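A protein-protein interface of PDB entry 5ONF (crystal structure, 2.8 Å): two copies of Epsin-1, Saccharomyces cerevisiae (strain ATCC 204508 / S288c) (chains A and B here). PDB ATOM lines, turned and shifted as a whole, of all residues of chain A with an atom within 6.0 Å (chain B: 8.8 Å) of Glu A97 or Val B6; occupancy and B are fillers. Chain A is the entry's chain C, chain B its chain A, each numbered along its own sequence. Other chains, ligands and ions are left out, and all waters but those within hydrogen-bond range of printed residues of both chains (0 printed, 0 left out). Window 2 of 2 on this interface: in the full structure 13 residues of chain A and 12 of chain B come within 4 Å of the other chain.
Glu A97 touches just these residues of chain B: Val B6 (3.1 Å) and Lys B10 (3.2 Å). Val B6 touches just one residue of chain A: Glu A97 (3.1 Å). Printed residues of chain A within 4 Å of Asn B29: Tyr A100 (3.4 Å). Printed residues of chain A within 4 Å of Ala B9: Phe A53 (3.9 Å). Of the printed residues of chain B, Phe A53 touches Ala B9 and Val B13. Printed residues of chain B within 4 Å of Asn A98: Lys B10 (3.1 Å). Val A92 touches none of the printed residues of chain B. Leu A93 touches none of the printed residues of chain B.
Printed residues of chain A that touch a printed residue of chain B: Phe A53, Trp A94, Glu A97, Asn A98 and Tyr A100. Hydrophobic or aromatic side chains of chain A within 4 Å of the printed part of chain B: Phe A53, Trp A94 and Tyr A100. Hydrophobic or aromatic side chains of chain B within 4 Å of the printed part of chain A: Val B6, Ala B9 and Val B13. Along chain B the printed residues that touch a printed residue of chain A span positions 6 to 29. Among the printed residues, 7 pairs touch across the chains. Among the printed residues, no Asp or Glu carboxylate lies within 4 Å of a Lys or Arg side-chain nitrogen of the other chain.
Phe A53 touches Ala B9. Phe A53 touches Val B13. Trp A94 touches Lys B10 (CH2 to CG, 3.6 Å). Glu A97 touches Val B6 (OE1 to CG1, 3.1 Å). Lys B10 touches Glu A97. CD1 of Tyr A100 touches ND2 of Asn B29 (3.4 Å).
The backbone NH (N) of Asn A98 lies close to the side-chain amino group (NZ) of Lys B10 (3.1 Å).
No position is printed for both chains.
The backbone carbonyl oxygen of Leu A93 lies close to the side-chain carboxylate of Glu A97. The backbone carbonyl oxygen (O) of Trp A94 lies close to the side-chain amide oxygen (OD1) of Asn A98 (2.9 Å). The backbone carbonyl oxygen (O) of Cys A95 sits close to the side-chain amide oxygen (OD1) of Asn A98 (3.1 Å).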
ATOM      1  N   PHE A  53      -0.307  11.901  -8.551  1.00  0.00           N
ATOM      2  CA  PHE A  53       0.684  10.842  -8.335  1.00  0.00           C
ATOM      3  C   PHE A  53       2.126  11.368  -8.223  1.00  0.00           C
ATOM      4  O   PHE A  53       2.921  10.836  -7.441  1.00  0.00           O
ATOM      5  CB  PHE A  53       0.549   9.762  -9.420  1.00  0.00           C
ATOM      6  CG  PHE A  53      -0.674   8.899  -9.251  1.00  0.00           C
ATOM      7  CD1 PHE A  53      -0.664   7.846  -8.341  1.00  0.00           C
ATOM      8  CD2 PHE A  53      -1.836   9.154  -9.957  1.00  0.00           C
ATOM      9  CE1 PHE A  53      -1.789   7.051  -8.159  1.00  0.00           C
ATOM     10  CE2 PHE A  53      -2.965   8.371  -9.779  1.00  0.00           C
ATOM     11  CZ  PHE A  53      -2.946   7.316  -8.883  1.00  0.00           C
ATOM     12  N   ASN A  90      -8.039  11.289  -2.020  1.00  0.00           N
ATOM     13  CA  ASN A  90      -7.051  10.383  -2.605  1.00  0.00           C
ATOM     14  C   ASN A  90      -5.715  10.433  -1.877  1.00  0.00           C
ATOM     15  O   ASN A  90      -5.092   9.390  -1.656  1.00  0.00           O
ATOM     16  CB  ASN A  90      -6.844  10.709  -4.087  1.00  0.00           C
ATOM     17  CG  ASN A  90      -8.059  10.380  -4.931  1.00  0.00           C
ATOM     18  OD1 ASN A  90      -8.592  11.231  -5.646  1.00  0.00           O
ATOM     19  ND2 ASN A  90      -8.505   9.138  -4.847  1.00  0.00           N
ATOM     20  N   VAL A  92      -5.097  11.282   1.344  1.00  0.00           N
ATOM     21  CA  VAL A  92      -5.142  10.713   2.686  1.00  0.00           C
ATOM     22  C   VAL A  92      -4.916   9.196   2.625  1.00  0.00           C
ATOM     23  O   VAL A  92      -4.078   8.663   3.362  1.00  0.00           O
ATOM     24  CB  VAL A  92      -6.468  11.036   3.415  1.00  0.00           C
ATOM     25  CG1 VAL A  92      -6.538  10.304   4.751  1.00  0.00           C
ATOM     26  CG2 VAL A  92      -6.611  12.539   3.640  1.00  0.00           C
ATOM     27  N   LEU A  93      -5.638   8.514   1.734  1.00  0.00           N
ATOM     28  CA  LEU A  93      -5.536   7.058   1.631  1.00  0.00           C
ATOM     29  C   LEU A  93      -4.166   6.612   1.128  1.00  0.00           C
ATOM     30  O   LEU A  93      -3.691   5.527   1.509  1.00  0.00           O
ATOM     31  CB  LEU A  93      -6.636   6.469   0.749  1.00  0.00           C
ATOM     32  CG  LEU A  93      -6.791   4.940   0.762  1.00  0.00           C
ATOM     33  CD1 LEU A  93      -7.056   4.408   2.166  1.00  0.00           C
ATOM     34  CD2 LEU A  93      -7.903   4.504  -0.190  1.00  0.00           C
ATOM     35  N   TRP A  94      -3.512   7.440   0.311  1.00  0.00           N
ATOM     36  CA  TRP A  94      -2.132   7.154  -0.071  1.00  0.00           C
ATOM     37  C   TRP A  94      -1.270   6.956   1.177  1.00  0.00           C
ATOM     38  O   TRP A  94      -0.549   5.952   1.294  1.00  0.00           O
ATOM     39  CB  TRP A  94      -1.559   8.271  -0.941  1.00  0.00           C
ATOM     40  CG  TRP A  94      -0.101   8.125  -1.208  1.00  0.00           C
ATOM     41  CD1 TRP A  94       0.918   8.515  -0.394  1.00  0.00           C
ATOM     42  CD2 TRP A  94       0.507   7.547  -2.365  1.00  0.00           C
ATOM     43  NE1 TRP A  94       2.127   8.211  -0.967  1.00  0.00           N
ATOM     44  CE2 TRP A  94       1.904   7.613  -2.178  1.00  0.00           C
ATOM     45  CE3 TRP A  94       0.008   6.976  -3.540  1.00  0.00           C
ATOM     46  CZ2 TRP A  94       2.813   7.143  -3.127  1.00  0.00           C
ATOM     47  CZ3 TRP A  94       0.910   6.506  -4.487  1.00  0.00           C
ATOM     48  CH2 TRP A  94       2.301   6.594  -4.272  1.00  0.00           C
ATOM     49  N   CYS A  95      -1.375   7.907   2.105  1.00  0.00           N
ATOM     50  CA  CYS A  95      -0.583   7.891   3.336  1.00  0.00           C
ATOM     51  C   CYS A  95      -0.831   6.667   4.218  1.00  0.00           C
ATOM     52  O   CYS A  95       0.106   6.140   4.809  1.00  0.00           O
ATOM     53  CB  CYS A  95      -0.810   9.167   4.129  1.00  0.00           C
ATOM     54  SG  CYS A  95      -0.369  10.634   3.177  1.00  0.00           S
ATOM     55  N   ARG A  96      -2.075   6.197   4.259  1.00  0.00           N
ATOM     56  CA  ARG A  96      -2.441   5.004   5.034  1.00  0.00           C
ATOM     57  C   ARG A  96      -1.656   3.744   4.627  1.00  0.00           C
ATOM     58  O   ARG A  96      -1.461   2.846   5.449  1.00  0.00           O
ATOM     59  CB  ARG A  96      -3.956   4.744   4.945  1.00  0.00           C
ATOM     60  CG  ARG A  96      -4.807   5.851   5.555  1.00  0.00           C
ATOM     61  CD  ARG A  96      -6.179   5.347   5.959  1.00  0.00           C
ATOM     62  NE  ARG A  96      -6.959   6.379   6.640  1.00  0.00           N
ATOM     63  CZ  ARG A  96      -8.110   6.167   7.280  1.00  0.00           C
ATOM     64  NH1 ARG A  96      -8.649   4.945   7.348  1.00  0.00           N
ATOM     65  NH2 ARG A  96      -8.735   7.190   7.862  1.00  0.00           N
ATOM     66  N   GLU A  97      -1.193   3.689   3.374  1.00  0.00           N
ATOM     67  CA  GLU A  97      -0.428   2.540   2.880  1.00  0.00           C
ATOM     68  C   GLU A  97       1.064   2.679   3.185  1.00  0.00           C
ATOM     69  O   GLU A  97       1.669   1.737   3.708  1.00  0.00           O
ATOM     70  CB  GLU A  97      -0.677   2.310   1.384  1.00  0.00           C
ATOM     71  CG  GLU A  97      -1.921   1.491   1.088  1.00  0.00           C
ATOM     72  CD  GLU A  97      -3.201   2.183   1.504  1.00  0.00           C
ATOM     73  OE1 GLU A  97      -3.753   2.943   0.686  1.00  0.00           O
ATOM     74  OE2 GLU A  97      -3.658   1.953   2.644  1.00  0.00           O
ATOM     75  N   ASN A  98       1.639   3.859   2.916  1.00  0.00           N
ATOM     76  CA  ASN A  98       3.056   4.133   3.245  1.00  0.00           C
ATOM     77  C   ASN A  98       3.171   4.751   4.649  1.00  0.00           C
ATOM     78  O   ASN A  98       3.953   5.683   4.888  1.00  0.00           O
ATOM     79  CB  ASN A  98       3.771   4.994   2.181  1.00  0.00           C
ATOM     80  CG  ASN A  98       3.221   6.401   2.066  1.00  0.00           C
ATOM     81  OD1 ASN A  98       2.076   6.666   2.415  1.00  0.00           O
ATOM     82  ND2 ASN A  98       4.047   7.314   1.569  1.00  0.00           N
ATOM     83  N   LEU A  99       2.387   4.208   5.579  1.00  0.00           N
ATOM     84  CA  LEU A  99       2.400   4.642   6.962  1.00  0.00           C
ATOM     85  C   LEU A  99       3.701   4.231   7.659  1.00  0.00           C
ATOM     86  O   LEU A  99       4.143   4.903   8.594  1.00  0.00           O
ATOM     87  CB  LEU A  99       1.200   4.041   7.702  1.00  0.00           C
ATOM     88  CG  LEU A  99       0.953   4.494   9.143  1.00  0.00           C
ATOM     89  CD1 LEU A  99       0.671   5.988   9.217  1.00  0.00           C
ATOM     90  CD2 LEU A  99      -0.206   3.710   9.740  1.00  0.00           C
ATOM     91  N   TYR A 100       4.293   3.123   7.208  1.00  0.00           N
ATOM     92  CA  TYR A 100       5.611   2.658   7.679  1.00  0.00           C
ATOM     93  C   TYR A 100       6.744   3.700   7.588  1.00  0.00           C
ATOM     94  O   TYR A 100       7.675   3.670   8.404  1.00  0.00           O
ATOM     95  CB  TYR A 100       6.025   1.359   6.950  1.00  0.00           C
ATOM     96  CG  TYR A 100       6.459   1.520   5.494  1.00  0.00           C
ATOM     97  CD1 TYR A 100       7.814   1.516   5.146  1.00  0.00           C
ATOM     98  CD2 TYR A 100       5.520   1.661   4.465  1.00  0.00           C
ATOM     99  CE1 TYR A 100       8.220   1.656   3.826  1.00  0.00           C
ATOM    100  CE2 TYR A 100       5.919   1.803   3.140  1.00  0.00           C
ATOM    101  CZ  TYR A 100       7.268   1.800   2.824  1.00  0.00           C
ATOM    102  OH  TYR A 100       7.666   1.940   1.517  1.00  0.00           O
ATOM    103  N   SER B   2     -11.439   5.754  -6.782  1.00  0.00           N
ATOM    104  CA  SER B   2     -11.064   4.351  -6.629  1.00  0.00           C
ATOM    105  C   SER B   2     -10.161   4.128  -5.405  1.00  0.00           C
ATOM    106  O   SER B   2      -9.617   5.089  -4.839  1.00  0.00           O
ATOM    107  CB  SER B   2     -10.399   3.845  -7.916  1.00  0.00           C
ATOM    108  OG  SER B   2     -11.274   3.986  -9.027  1.00  0.00           O
ATOM    109  N   LYS B   3     -10.012   2.860  -5.009  1.00  0.00           N
ATOM    110  CA  LYS B   3      -9.581   2.497  -3.642  1.00  0.00           C
ATOM    111  C   LYS B   3      -8.449   1.462  -3.540  1.00  0.00           C
ATOM    112  O   LYS B   3      -7.292   1.838  -3.444  1.00  0.00           O
ATOM    113  CB  LYS B   3     -10.794   1.992  -2.846  1.00  0.00           C
ATOM    114  CG  LYS B   3     -11.941   2.976  -2.730  1.00  0.00           C
ATOM    115  CD  LYS B   3     -13.167   2.312  -2.121  1.00  0.00           C
ATOM    116  CE  LYS B   3     -14.366   3.245  -2.161  1.00  0.00           C
ATOM    117  NZ  LYS B   3     -14.133   4.505  -1.398  1.00  0.00           N
ATOM    118  N   GLN B   4      -8.796   0.171  -3.578  1.00  0.00           N
ATOM    119  CA  GLN B   4      -7.911  -0.938  -3.143  1.00  0.00           C
ATOM    120  C   GLN B   4      -6.692  -1.212  -4.037  1.00  0.00           C
ATOM    121  O   GLN B   4      -5.675  -1.728  -3.565  1.00  0.00           O
ATOM    122  CB  GLN B   4      -8.710  -2.245  -2.947  1.00  0.00           C
ATOM    123  CG  GLN B   4      -9.585  -2.676  -4.129  1.00  0.00           C
ATOM    124  CD  GLN B   4     -10.082  -4.115  -4.058  1.00  0.00           C
ATOM    125  OE1 GLN B   4     -11.148  -4.431  -4.594  1.00  0.00           O
ATOM    126  NE2 GLN B   4      -9.317  -4.996  -3.413  1.00  0.00           N
ATOM    127  N   PHE B   5      -6.801  -0.870  -5.319  1.00  0.00           N
ATOM    128  CA  PHE B   5      -5.658  -0.900  -6.249  1.00  0.00           C
ATOM    129  C   PHE B   5      -4.482   0.012  -5.852  1.00  0.00           C
ATOM    130  O   PHE B   5      -3.372  -0.159  -6.375  1.00  0.00           O
ATOM    131  CB  PHE B   5      -6.103  -0.486  -7.658  1.00  0.00           C
ATOM    132  CG  PHE B   5      -6.119   1.008  -7.868  1.00  0.00           C
ATOM    133  CD1 PHE B   5      -5.176   1.627  -8.689  1.00  0.00           C
ATOM    134  CD2 PHE B   5      -7.053   1.806  -7.206  1.00  0.00           C
ATOM    135  CE1 PHE B   5      -5.185   3.005  -8.868  1.00  0.00           C
ATOM    136  CE2 PHE B   5      -7.060   3.183  -7.379  1.00  0.00           C
ATOM    137  CZ  PHE B   5      -6.127   3.784  -8.210  1.00  0.00           C
ATOM    138  N   VAL B   6      -4.739   0.995  -4.978  1.00  0.00           N
ATOM    139  CA  VAL B   6      -3.749   2.016  -4.595  1.00  0.00           C
ATOM    140  C   VAL B   6      -2.401   1.453  -4.119  1.00  0.00           C
ATOM    141  O   VAL B   6      -1.365   2.113  -4.275  1.00  0.00           O
ATOM    142  CB  VAL B   6      -4.313   2.988  -3.523  1.00  0.00           C
ATOM    143  CG1 VAL B   6      -4.584   2.269  -2.203  1.00  0.00           C
ATOM    144  CG2 VAL B   6      -3.380   4.176  -3.311  1.00  0.00           C
ATOM    145  N   ARG B   7      -2.413   0.258  -3.529  1.00  0.00           N
ATOM    146  CA  ARG B   7      -1.172  -0.454  -3.250  1.00  0.00           C
ATOM    147  C   ARG B   7      -0.364  -0.608  -4.545  1.00  0.00           C
ATOM    148  O   ARG B   7       0.789  -0.177  -4.618  1.00  0.00           O
ATOM    149  CB  ARG B   7      -1.461  -1.818  -2.606  1.00  0.00           C
ATOM    150  CG  ARG B   7      -0.253  -2.734  -2.440  1.00  0.00           C
ATOM    151  CD  ARG B   7       0.832  -2.141  -1.547  1.00  0.00           C
ATOM    152  NE  ARG B   7       2.134  -2.787  -1.758  1.00  0.00           N
ATOM    153  CZ  ARG B   7       3.113  -2.352  -2.564  1.00  0.00           C
ATOM    154  NH1 ARG B   7       2.990  -1.234  -3.284  1.00  0.00           N
ATOM    155  NH2 ARG B   7       4.247  -3.050  -2.649  1.00  0.00           N
ATOM    156  N   SER B   8      -0.997  -1.186  -5.566  1.00  0.00           N
ATOM    157  CA  SER B   8      -0.364  -1.401  -6.879  1.00  0.00           C
ATOM    158  C   SER B   8      -0.226  -0.140  -7.748  1.00  0.00           C
ATOM    159  O   SER B   8       0.537  -0.141  -8.724  1.00  0.00           O
ATOM    160  CB  SER B   8      -1.119  -2.471  -7.665  1.00  0.00           C
ATOM    161  OG  SER B   8      -0.503  -2.678  -8.921  1.00  0.00           O
ATOM    162  N   ALA B   9      -0.972   0.912  -7.416  1.00  0.00           N
ATOM    163  CA  ALA B   9      -0.778   2.226  -8.028  1.00  0.00           C
ATOM    164  C   ALA B   9       0.617   2.781  -7.779  1.00  0.00           C
ATOM    165  O   ALA B   9       1.157   3.481  -8.621  1.00  0.00           O
ATOM    166  CB  ALA B   9      -1.827   3.206  -7.527  1.00  0.00           C
ATOM    167  N   LYS B  10       1.198   2.442  -6.632  1.00  0.00           N
ATOM    168  CA  LYS B  10       2.529   2.930  -6.235  1.00  0.00           C
ATOM    169  C   LYS B  10       3.643   2.342  -7.079  1.00  0.00           C
ATOM    170  O   LYS B  10       4.553   3.057  -7.516  1.00  0.00           O
ATOM    171  CB  LYS B  10       2.823   2.561  -4.795  1.00  0.00           C
ATOM    172  CG  LYS B  10       1.810   3.067  -3.793  1.00  0.00           C
ATOM    173  CD  LYS B  10       2.256   2.773  -2.384  1.00  0.00           C
ATOM    174  CE  LYS B  10       1.389   3.511  -1.393  1.00  0.00           C
ATOM    175  NZ  LYS B  10       2.010   3.313  -0.077  1.00  0.00           N
ATOM    176  N   ASN B  11       3.563   1.028  -7.292  1.00  0.00           N
ATOM    177  CA  ASN B  11       4.601   0.284  -8.004  1.00  0.00           C
ATOM    178  C   ASN B  11       4.663   0.682  -9.465  1.00  0.00           C
ATOM    179  O   ASN B  11       5.726   0.649 -10.102  1.00  0.00           O
ATOM    180  CB  ASN B  11       4.329  -1.209  -7.900  1.00  0.00           C
ATOM    181  CG  ASN B  11       4.110  -1.655  -6.472  1.00  0.00           C
ATOM    182  OD1 ASN B  11       2.978  -1.684  -5.992  1.00  0.00           O
ATOM    183  ND2 ASN B  11       5.194  -1.950  -5.770  1.00  0.00           N
ATOM    184  N   LEU B  12       3.500   1.055  -9.985  1.00  0.00           N
ATOM    185  CA  LEU B  12       3.381   1.535 -11.351  1.00  0.00           C
ATOM    186  C   LEU B  12       4.060   2.886 -11.537  1.00  0.00           C
ATOM    187  O   LEU B  12       4.720   3.099 -12.556  1.00  0.00           O
ATOM    188  CB  LEU B  12       1.909   1.639 -11.748  1.00  0.00           C
ATOM    189  CG  LEU B  12       1.613   1.765 -13.241  1.00  0.00           C
ATOM    190  CD1 LEU B  12       2.293   0.673 -14.066  1.00  0.00           C
ATOM    191  CD2 LEU B  12       0.109   1.704 -13.435  1.00  0.00           C
ATOM    192  N   VAL B  13       3.922   3.774 -10.546  1.00  0.00           N
ATOM    193  CA  VAL B  13       4.535   5.111 -10.603  1.00  0.00           C
ATOM    194  C   VAL B  13       6.046   4.983 -10.845  1.00  0.00           C
ATOM    195  O   VAL B  13       6.580   5.620 -11.753  1.00  0.00           O
ATOM    196  CB  VAL B  13       4.255   5.958  -9.329  1.00  0.00           C
ATOM    197  CG1 VAL B  13       4.978   7.300  -9.387  1.00  0.00           C
ATOM    198  CG2 VAL B  13       2.761   6.209  -9.164  1.00  0.00           C
ATOM    199  N   ASN B  29       9.634  -4.520   4.873  1.00  0.00           N
ATOM    200  CA  ASN B  29      10.190  -3.760   5.997  1.00  0.00           C
ATOM    201  C   ASN B  29       9.648  -4.163   7.374  1.00  0.00           C
ATOM    202  O   ASN B  29       9.828  -3.410   8.337  1.00  0.00           O
ATOM    203  CB  ASN B  29       9.960  -2.258   5.761  1.00  0.00           C
ATOM    204  CG  ASN B  29       8.532  -1.821   6.045  1.00  0.00           C
ATOM    205  OD1 ASN B  29       7.624  -2.069   5.253  1.00  0.00           O
ATOM    206  ND2 ASN B  29       8.337  -1.157   7.174  1.00  0.00           N
ATOM    207  N   ASP B  30       9.023  -5.339   7.486  1.00  0.00           N
ATOM    208  CA  ASP B  30       8.330  -5.732   8.725  1.00  0.00           C
ATOM    209  C   ASP B  30       9.218  -6.519   9.704  1.00  0.00           C
ATOM    210  O   ASP B  30       9.721  -5.937  10.661  1.00  0.00           O
ATOM    211  CB  ASP B  30       7.020  -6.485   8.415  1.00  0.00           C
ATOM    212  CG  ASP B  30       5.855  -5.550   8.064  1.00  0.00           C
ATOM    213  OD1 ASP B  30       6.056  -4.318   7.930  1.00  0.00           O
ATOM    214  OD2 ASP B  30       4.723  -6.062   7.920  1.00  0.00           O
